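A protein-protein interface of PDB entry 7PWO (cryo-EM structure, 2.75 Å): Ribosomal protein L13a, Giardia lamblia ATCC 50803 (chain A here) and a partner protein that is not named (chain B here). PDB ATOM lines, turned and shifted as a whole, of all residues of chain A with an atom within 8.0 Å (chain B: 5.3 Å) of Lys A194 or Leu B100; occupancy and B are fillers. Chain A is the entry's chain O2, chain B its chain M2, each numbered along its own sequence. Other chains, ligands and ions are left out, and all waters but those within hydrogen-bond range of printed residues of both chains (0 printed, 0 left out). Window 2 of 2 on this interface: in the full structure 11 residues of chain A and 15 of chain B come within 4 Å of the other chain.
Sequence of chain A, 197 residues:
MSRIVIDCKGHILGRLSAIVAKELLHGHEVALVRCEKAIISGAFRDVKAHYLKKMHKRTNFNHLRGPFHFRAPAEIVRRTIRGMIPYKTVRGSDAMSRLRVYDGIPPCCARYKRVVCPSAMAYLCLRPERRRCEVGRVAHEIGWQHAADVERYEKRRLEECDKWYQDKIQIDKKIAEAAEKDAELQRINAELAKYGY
The side-chain carboxylate (OE2) of Glu A191 lies close to the backbone carbonyl oxygen (O) of Leu B115, at 3.4 Å. O of Lys A194 sits close to O of Leu B100.
The backbone carbonyl oxygen (O) of Gln B97 sits at hydrogen-bond distance from the guanidinium group (NE) of Arg B101 (3.5 Å). The side-chain carboxylate (OE1) of Glu A191 is in hydrogen-bond range of the side-chain hydroxyl (OH) of Tyr A195 (2.7 Å).
Among the printed residues, pairs that only touch across the chains: Tyr A195 with Leu B100 (3.0 Å), Tyr A195 with Gln B97 (3.3 Å), Lys A194 with Arg B101 (3.6 Å), Ala A193 with Leu B100 (3.7 Å), Lys A194 with Ile B112 (3.8 Å), Tyr A195 with Arg B101 (3.9 Å), Lys A194 with Asp B108 (3.9 Å) and Lys A194 with Lys B111 (3.96 Å).
Lys A194 touches just these residues of chain B: Leu B100, Arg B101, Asp B108, Lys B111 and Ile B112. Printed residues of chain A within 4 Å of Leu B100: Ala A193 (3.7 Å), Lys A194 (3.0 Å) and Tyr A195 (3.0 Å). Printed residues of chain A within 4 Å of Arg B101: Lys A194 and Tyr A195. Printed residues of chain B within 4 Å of Tyr A195: Gln B97 (3.3 Å), Leu B100 (3.0 Å) and Arg B101 (3.9 Å). The nearest printed residue of chain B that does not touch Lys A194 is Leu B115 (5.1 Å). The nearest residue of chain A that does not touch Leu B100 is Leu A192 (4.5 Å). The nearest printed residue of chain A that does not touch Leu B115 is Ala A190 (4.1 Å).
Of the 8 printed residues of chain A, 4 touch a printed residue of chain B. Hydrophobic or aromatic side chains of chain B that line the printed part of chain A: Leu B100, Ile B112 and Leu B115. Along chain B the printed residues that touch a printed residue of chain A span positions 97 to 115.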
ATOM      1  N   ILE A 188      -7.763  21.565  -6.969  1.00  0.00           N
ATOM      2  CA  ILE A 188      -8.751  21.162  -5.965  1.00  0.00           C
ATOM      3  C   ILE A 188      -8.688  22.102  -4.774  1.00  0.00           C
ATOM      4  O   ILE A 188      -9.718  22.428  -4.170  1.00  0.00           O
ATOM      5  CB  ILE A 188      -8.556  19.694  -5.545  1.00  0.00           C
ATOM      6  CG1 ILE A 188      -8.951  18.756  -6.680  1.00  0.00           C
ATOM      7  CG2 ILE A 188      -9.390  19.359  -4.315  1.00  0.00           C
ATOM      8  CD1 ILE A 188     -10.326  19.014  -7.221  1.00  0.00           C
ATOM      9  N   ASN A 189      -7.492  22.590  -4.442  1.00  0.00           N
ATOM     10  CA  ASN A 189      -7.400  23.633  -3.422  1.00  0.00           C
ATOM     11  C   ASN A 189      -8.165  24.893  -3.837  1.00  0.00           C
ATOM     12  O   ASN A 189      -8.803  25.551  -3.003  1.00  0.00           O
ATOM     13  CB  ASN A 189      -5.940  23.964  -3.145  1.00  0.00           C
ATOM     14  CG  ASN A 189      -5.775  25.081  -2.130  1.00  0.00           C
ATOM     15  OD1 ASN A 189      -6.535  25.186  -1.164  1.00  0.00           O
ATOM     16  ND2 ASN A 189      -4.794  25.938  -2.362  1.00  0.00           N
ATOM     17  N   ALA A 190      -8.095  25.263  -5.118  1.00  0.00           N
ATOM     18  CA  ALA A 190      -8.827  26.437  -5.581  1.00  0.00           C
ATOM     19  C   ALA A 190     -10.330  26.201  -5.539  1.00  0.00           C
ATOM     20  O   ALA A 190     -11.101  27.103  -5.188  1.00  0.00           O
ATOM     21  CB  ALA A 190      -8.391  26.811  -6.992  1.00  0.00           C
ATOM     22  N   GLU A 191     -10.765  25.002  -5.928  1.00  0.00           N
ATOM     23  CA  GLU A 191     -12.156  24.631  -5.735  1.00  0.00           C
ATOM     24  C   GLU A 191     -12.562  24.844  -4.288  1.00  0.00           C
ATOM     25  O   GLU A 191     -13.629  25.406  -4.006  1.00  0.00           O
ATOM     26  CB  GLU A 191     -12.383  23.171  -6.103  1.00  0.00           C
ATOM     27  CG  GLU A 191     -12.185  22.815  -7.554  1.00  0.00           C
ATOM     28  CD  GLU A 191     -13.189  23.453  -8.460  1.00  0.00           C
ATOM     29  OE1 GLU A 191     -14.339  23.679  -8.045  1.00  0.00           O
ATOM     30  OE2 GLU A 191     -12.826  23.676  -9.626  1.00  0.00           O
ATOM     31  N   LEU A 192     -11.715  24.395  -3.356  1.00  0.00           N
ATOM     32  CA  LEU A 192     -12.052  24.481  -1.941  1.00  0.00           C
ATOM     33  C   LEU A 192     -12.195  25.922  -1.489  1.00  0.00           C
ATOM     34  O   LEU A 192     -13.057  26.237  -0.663  1.00  0.00           O
ATOM     35  CB  LEU A 192     -11.006  23.765  -1.089  1.00  0.00           C
ATOM     36  CG  LEU A 192     -11.119  22.239  -1.071  1.00  0.00           C
ATOM     37  CD1 LEU A 192     -10.163  21.615  -0.063  1.00  0.00           C
ATOM     38  CD2 LEU A 192     -12.563  21.795  -0.841  1.00  0.00           C
ATOM     39  N   ALA A 193     -11.336  26.806  -1.993  1.00  0.00           N
ATOM     40  CA  ALA A 193     -11.447  28.213  -1.614  1.00  0.00           C
ATOM     41  C   ALA A 193     -12.856  28.738  -1.862  1.00  0.00           C
ATOM     42  O   ALA A 193     -13.395  29.501  -1.053  1.00  0.00           O
ATOM     43  CB  ALA A 193     -10.425  29.049  -2.371  1.00  0.00           C
ATOM     44  N   LYS A 194     -13.480  28.325  -2.969  1.00  0.00           N
ATOM     45  CA  LYS A 194     -14.802  28.837  -3.308  1.00  0.00           C
ATOM     46  C   LYS A 194     -15.929  28.043  -2.662  1.00  0.00           C
ATOM     47  O   LYS A 194     -16.985  28.614  -2.376  1.00  0.00           O
ATOM     48  CB  LYS A 194     -14.988  28.851  -4.825  1.00  0.00           C
ATOM     49  CG  LYS A 194     -14.070  29.793  -5.586  1.00  0.00           C
ATOM     50  CD  LYS A 194     -14.060  31.194  -4.994  1.00  0.00           C
ATOM     51  CE  LYS A 194     -13.543  32.199  -5.996  1.00  0.00           C
ATOM     52  NZ  LYS A 194     -12.301  31.726  -6.643  1.00  0.00           N
ATOM     53  N   TYR A 195     -15.749  26.746  -2.426  1.00  0.00           N
ATOM     54  CA  TYR A 195     -16.847  25.950  -1.872  1.00  0.00           C
ATOM     55  C   TYR A 195     -17.058  26.206  -0.394  1.00  0.00           C
ATOM     56  O   TYR A 195     -16.145  26.635   0.304  1.00  0.00           O
ATOM     57  CB  TYR A 195     -16.617  24.452  -2.102  1.00  0.00           C
ATOM     58  CG  TYR A 195     -16.669  24.062  -3.553  1.00  0.00           C
ATOM     59  CD1 TYR A 195     -17.679  24.537  -4.370  1.00  0.00           C
ATOM     60  CD2 TYR A 195     -15.725  23.215  -4.103  1.00  0.00           C
ATOM     61  CE1 TYR A 195     -17.754  24.198  -5.684  1.00  0.00           C
ATOM     62  CE2 TYR A 195     -15.794  22.860  -5.435  1.00  0.00           C
ATOM     63  CZ  TYR A 195     -16.815  23.360  -6.221  1.00  0.00           C
ATOM     64  OH  TYR A 195     -16.915  23.025  -7.552  1.00  0.00           O
ATOM     65  N   GLN B  96     -20.759  23.896   6.299  1.00  0.00           N
ATOM     66  CA  GLN B  96     -19.710  24.908   6.267  1.00  0.00           C
ATOM     67  C   GLN B  96     -19.398  25.317   4.836  1.00  0.00           C
ATOM     68  O   GLN B  96     -19.240  26.507   4.545  1.00  0.00           O
ATOM     69  CB  GLN B  96     -18.447  24.410   6.963  1.00  0.00           C
ATOM     70  CG  GLN B  96     -18.590  24.204   8.450  1.00  0.00           C
ATOM     71  CD  GLN B  96     -17.320  23.694   9.083  1.00  0.00           C
ATOM     72  OE1 GLN B  96     -16.335  23.431   8.398  1.00  0.00           O
ATOM     73  NE2 GLN B  96     -17.346  23.517  10.397  1.00  0.00           N
ATOM     74  N   GLN B  97     -19.302  24.344   3.928  1.00  0.00           N
ATOM     75  CA  GLN B  97     -19.009  24.719   2.550  1.00  0.00           C
ATOM     76  C   GLN B  97     -20.225  25.255   1.794  1.00  0.00           C
ATOM     77  O   GLN B  97     -20.057  26.046   0.856  1.00  0.00           O
ATOM     78  CB  GLN B  97     -18.343  23.564   1.799  1.00  0.00           C
ATOM     79  CG  GLN B  97     -19.146  22.296   1.584  1.00  0.00           C
ATOM     80  CD  GLN B  97     -18.316  21.236   0.873  1.00  0.00           C
ATOM     81  OE1 GLN B  97     -18.782  20.123   0.659  1.00  0.00           O
ATOM     82  NE2 GLN B  97     -17.090  21.579   0.506  1.00  0.00           N
ATOM     83  N   GLN B  98     -21.442  24.900   2.204  1.00  0.00           N
ATOM     84  CA  GLN B  98     -22.604  25.601   1.674  1.00  0.00           C
ATOM     85  C   GLN B  98     -22.666  27.053   2.137  1.00  0.00           C
ATOM     86  O   GLN B  98     -23.496  27.812   1.635  1.00  0.00           O
ATOM     87  CB  GLN B  98     -23.894  24.877   2.077  1.00  0.00           C
ATOM     88  CG  GLN B  98     -24.336  23.765   1.139  1.00  0.00           C
ATOM     89  CD  GLN B  98     -25.331  22.806   1.777  1.00  0.00           C
ATOM     90  OE1 GLN B  98     -25.786  23.020   2.903  1.00  0.00           O
ATOM     91  NE2 GLN B  98     -25.669  21.744   1.062  1.00  0.00           N
ATOM     92  N   ARG B  99     -21.835  27.442   3.099  1.00  0.00           N
ATOM     93  CA  ARG B  99     -21.753  28.839   3.514  1.00  0.00           C
ATOM     94  C   ARG B  99     -20.686  29.647   2.783  1.00  0.00           C
ATOM     95  O   ARG B  99     -20.826  30.867   2.682  1.00  0.00           O
ATOM     96  CB  ARG B  99     -21.490  28.926   5.018  1.00  0.00           C
ATOM     97  CG  ARG B  99     -22.593  28.315   5.835  1.00  0.00           C
ATOM     98  CD  ARG B  99     -22.285  28.339   7.292  1.00  0.00           C
ATOM     99  NE  ARG B  99     -23.429  27.899   8.084  1.00  0.00           N
ATOM    100  CZ  ARG B  99     -23.379  27.651   9.385  1.00  0.00           C
ATOM    101  NH1 ARG B  99     -22.235  27.796  10.037  1.00  0.00           N
ATOM    102  NH2 ARG B  99     -24.468  27.258  10.030  1.00  0.00           N
ATOM    103  N   LEU B 100     -19.622  29.016   2.274  1.00  0.00           N
ATOM    104  CA  LEU B 100     -18.698  29.734   1.400  1.00  0.00           C
ATOM    105  C   LEU B 100     -19.133  29.695  -0.054  1.00  0.00           C
ATOM    106  O   LEU B 100     -18.697  30.547  -0.833  1.00  0.00           O
ATOM    107  CB  LEU B 100     -17.279  29.177   1.503  1.00  0.00           C
ATOM    108  CG  LEU B 100     -16.363  29.506   2.673  1.00  0.00           C
ATOM    109  CD1 LEU B 100     -16.824  28.811   3.935  1.00  0.00           C
ATOM    110  CD2 LEU B 100     -14.927  29.103   2.319  1.00  0.00           C
ATOM    111  N   ARG B 101     -19.975  28.737  -0.445  1.00  0.00           N
ATOM    112  CA  ARG B 101     -20.554  28.808  -1.780  1.00  0.00           C
ATOM    113  C   ARG B 101     -21.825  29.641  -1.806  1.00  0.00           C
ATOM    114  O   ARG B 101     -22.393  29.846  -2.883  1.00  0.00           O
ATOM    115  CB  ARG B 101     -20.849  27.409  -2.344  1.00  0.00           C
ATOM    116  CG  ARG B 101     -22.142  26.790  -1.862  1.00  0.00           C
ATOM    117  CD  ARG B 101     -22.337  25.363  -2.353  1.00  0.00           C
ATOM    118  NE  ARG B 101     -21.254  24.451  -2.018  1.00  0.00           N
ATOM    119  CZ  ARG B 101     -21.307  23.131  -2.188  1.00  0.00           C
ATOM    120  NH1 ARG B 101     -22.393  22.559  -2.680  1.00  0.00           N
ATOM    121  NH2 ARG B 101     -20.275  22.376  -1.855  1.00  0.00           N
ATOM    122  N   ALA B 102     -22.284  30.116  -0.647  1.00  0.00           N
ATOM    123  CA  ALA B 102     -23.489  30.939  -0.584  1.00  0.00           C
ATOM    124  C   ALA B 102     -23.245  32.358  -1.083  1.00  0.00           C
ATOM    125  O   ALA B 102     -24.095  32.929  -1.772  1.00  0.00           O
ATOM    126  CB  ALA B 102     -24.016  30.971   0.846  1.00  0.00           C
ATOM    127  N   LYS B 103     -22.110  32.955  -0.726  1.00  0.00           N
ATOM    128  CA  LYS B 103     -21.884  34.388  -0.917  1.00  0.00           C
ATOM    129  C   LYS B 103     -21.051  34.652  -2.177  1.00  0.00           C
ATOM    130  O   LYS B 103     -19.942  35.191  -2.142  1.00  0.00           O
ATOM    131  CB  LYS B 103     -21.227  34.979   0.337  1.00  0.00           C
ATOM    132  CG  LYS B 103     -19.813  34.463   0.633  1.00  0.00           C
ATOM    133  CD  LYS B 103     -19.200  35.113   1.864  1.00  0.00           C
ATOM    134  CE  LYS B 103     -19.828  34.616   3.146  1.00  0.00           C
ATOM    135  NZ  LYS B 103     -19.475  33.183   3.284  1.00  0.00           N
ATOM    136  N   ASP B 108     -17.311  35.469  -9.653  1.00  0.00           N
ATOM    137  CA  ASP B 108     -17.010  34.224  -8.959  1.00  0.00           C
ATOM    138  C   ASP B 108     -17.597  33.028  -9.687  1.00  0.00           C
ATOM    139  O   ASP B 108     -16.952  31.980  -9.770  1.00  0.00           O
ATOM    140  CB  ASP B 108     -17.525  34.266  -7.524  1.00  0.00           C
ATOM    141  CG  ASP B 108     -16.946  35.401  -6.729  1.00  0.00           C
ATOM    142  OD1 ASP B 108     -17.420  36.538  -6.899  1.00  0.00           O
ATOM    143  OD2 ASP B 108     -16.038  35.156  -5.911  1.00  0.00           O
ATOM    144  N   LYS B 111     -15.384  32.159 -12.488  1.00  0.00           N
ATOM    145  CA  LYS B 111     -14.193  31.472 -11.994  1.00  0.00           C
ATOM    146  C   LYS B 111     -14.479  30.001 -11.704  1.00  0.00           C
ATOM    147  O   LYS B 111     -13.779  29.102 -12.195  1.00  0.00           O
ATOM    148  CB  LYS B 111     -13.705  32.180 -10.739  1.00  0.00           C
ATOM    149  CG  LYS B 111     -13.207  33.588 -10.985  1.00  0.00           C
ATOM    150  CD  LYS B 111     -12.742  34.207  -9.692  1.00  0.00           C
ATOM    151  CE  LYS B 111     -12.153  35.577  -9.903  1.00  0.00           C
ATOM    152  NZ  LYS B 111     -13.152  36.570 -10.351  1.00  0.00           N
ATOM    153  N   ILE B 112     -15.522  29.743 -10.912  1.00  0.00           N
ATOM    154  CA  ILE B 112     -15.858  28.381 -10.517  1.00  0.00           C
ATOM    155  C   ILE B 112     -16.217  27.543 -11.730  1.00  0.00           C
ATOM    156  O   ILE B 112     -15.941  26.339 -11.760  1.00  0.00           O
ATOM    157  CB  ILE B 112     -16.994  28.385  -9.470  1.00  0.00           C
ATOM    158  CG1 ILE B 112     -16.651  29.312  -8.308  1.00  0.00           C
ATOM    159  CG2 ILE B 112     -17.215  27.004  -8.916  1.00  0.00           C
ATOM    160  CD1 ILE B 112     -17.836  29.875  -7.598  1.00  0.00           C
ATOM    161  N   LEU B 115     -13.051  26.519 -13.551  1.00  0.00           N
ATOM    162  CA  LEU B 115     -12.371  25.511 -12.747  1.00  0.00           C
ATOM    163  C   LEU B 115     -13.051  24.148 -12.858  1.00  0.00           C
ATOM    164  O   LEU B 115     -12.378  23.120 -12.998  1.00  0.00           O
ATOM    165  CB  LEU B 115     -12.282  25.969 -11.295  1.00  0.00           C
ATOM    166  CG  LEU B 115     -11.409  27.196 -11.042  1.00  0.00           C
ATOM    167  CD1 LEU B 115     -11.456  27.586  -9.577  1.00  0.00           C
ATOM    168  CD2 LEU B 115      -9.994  26.934 -11.483  1.00  0.00           C
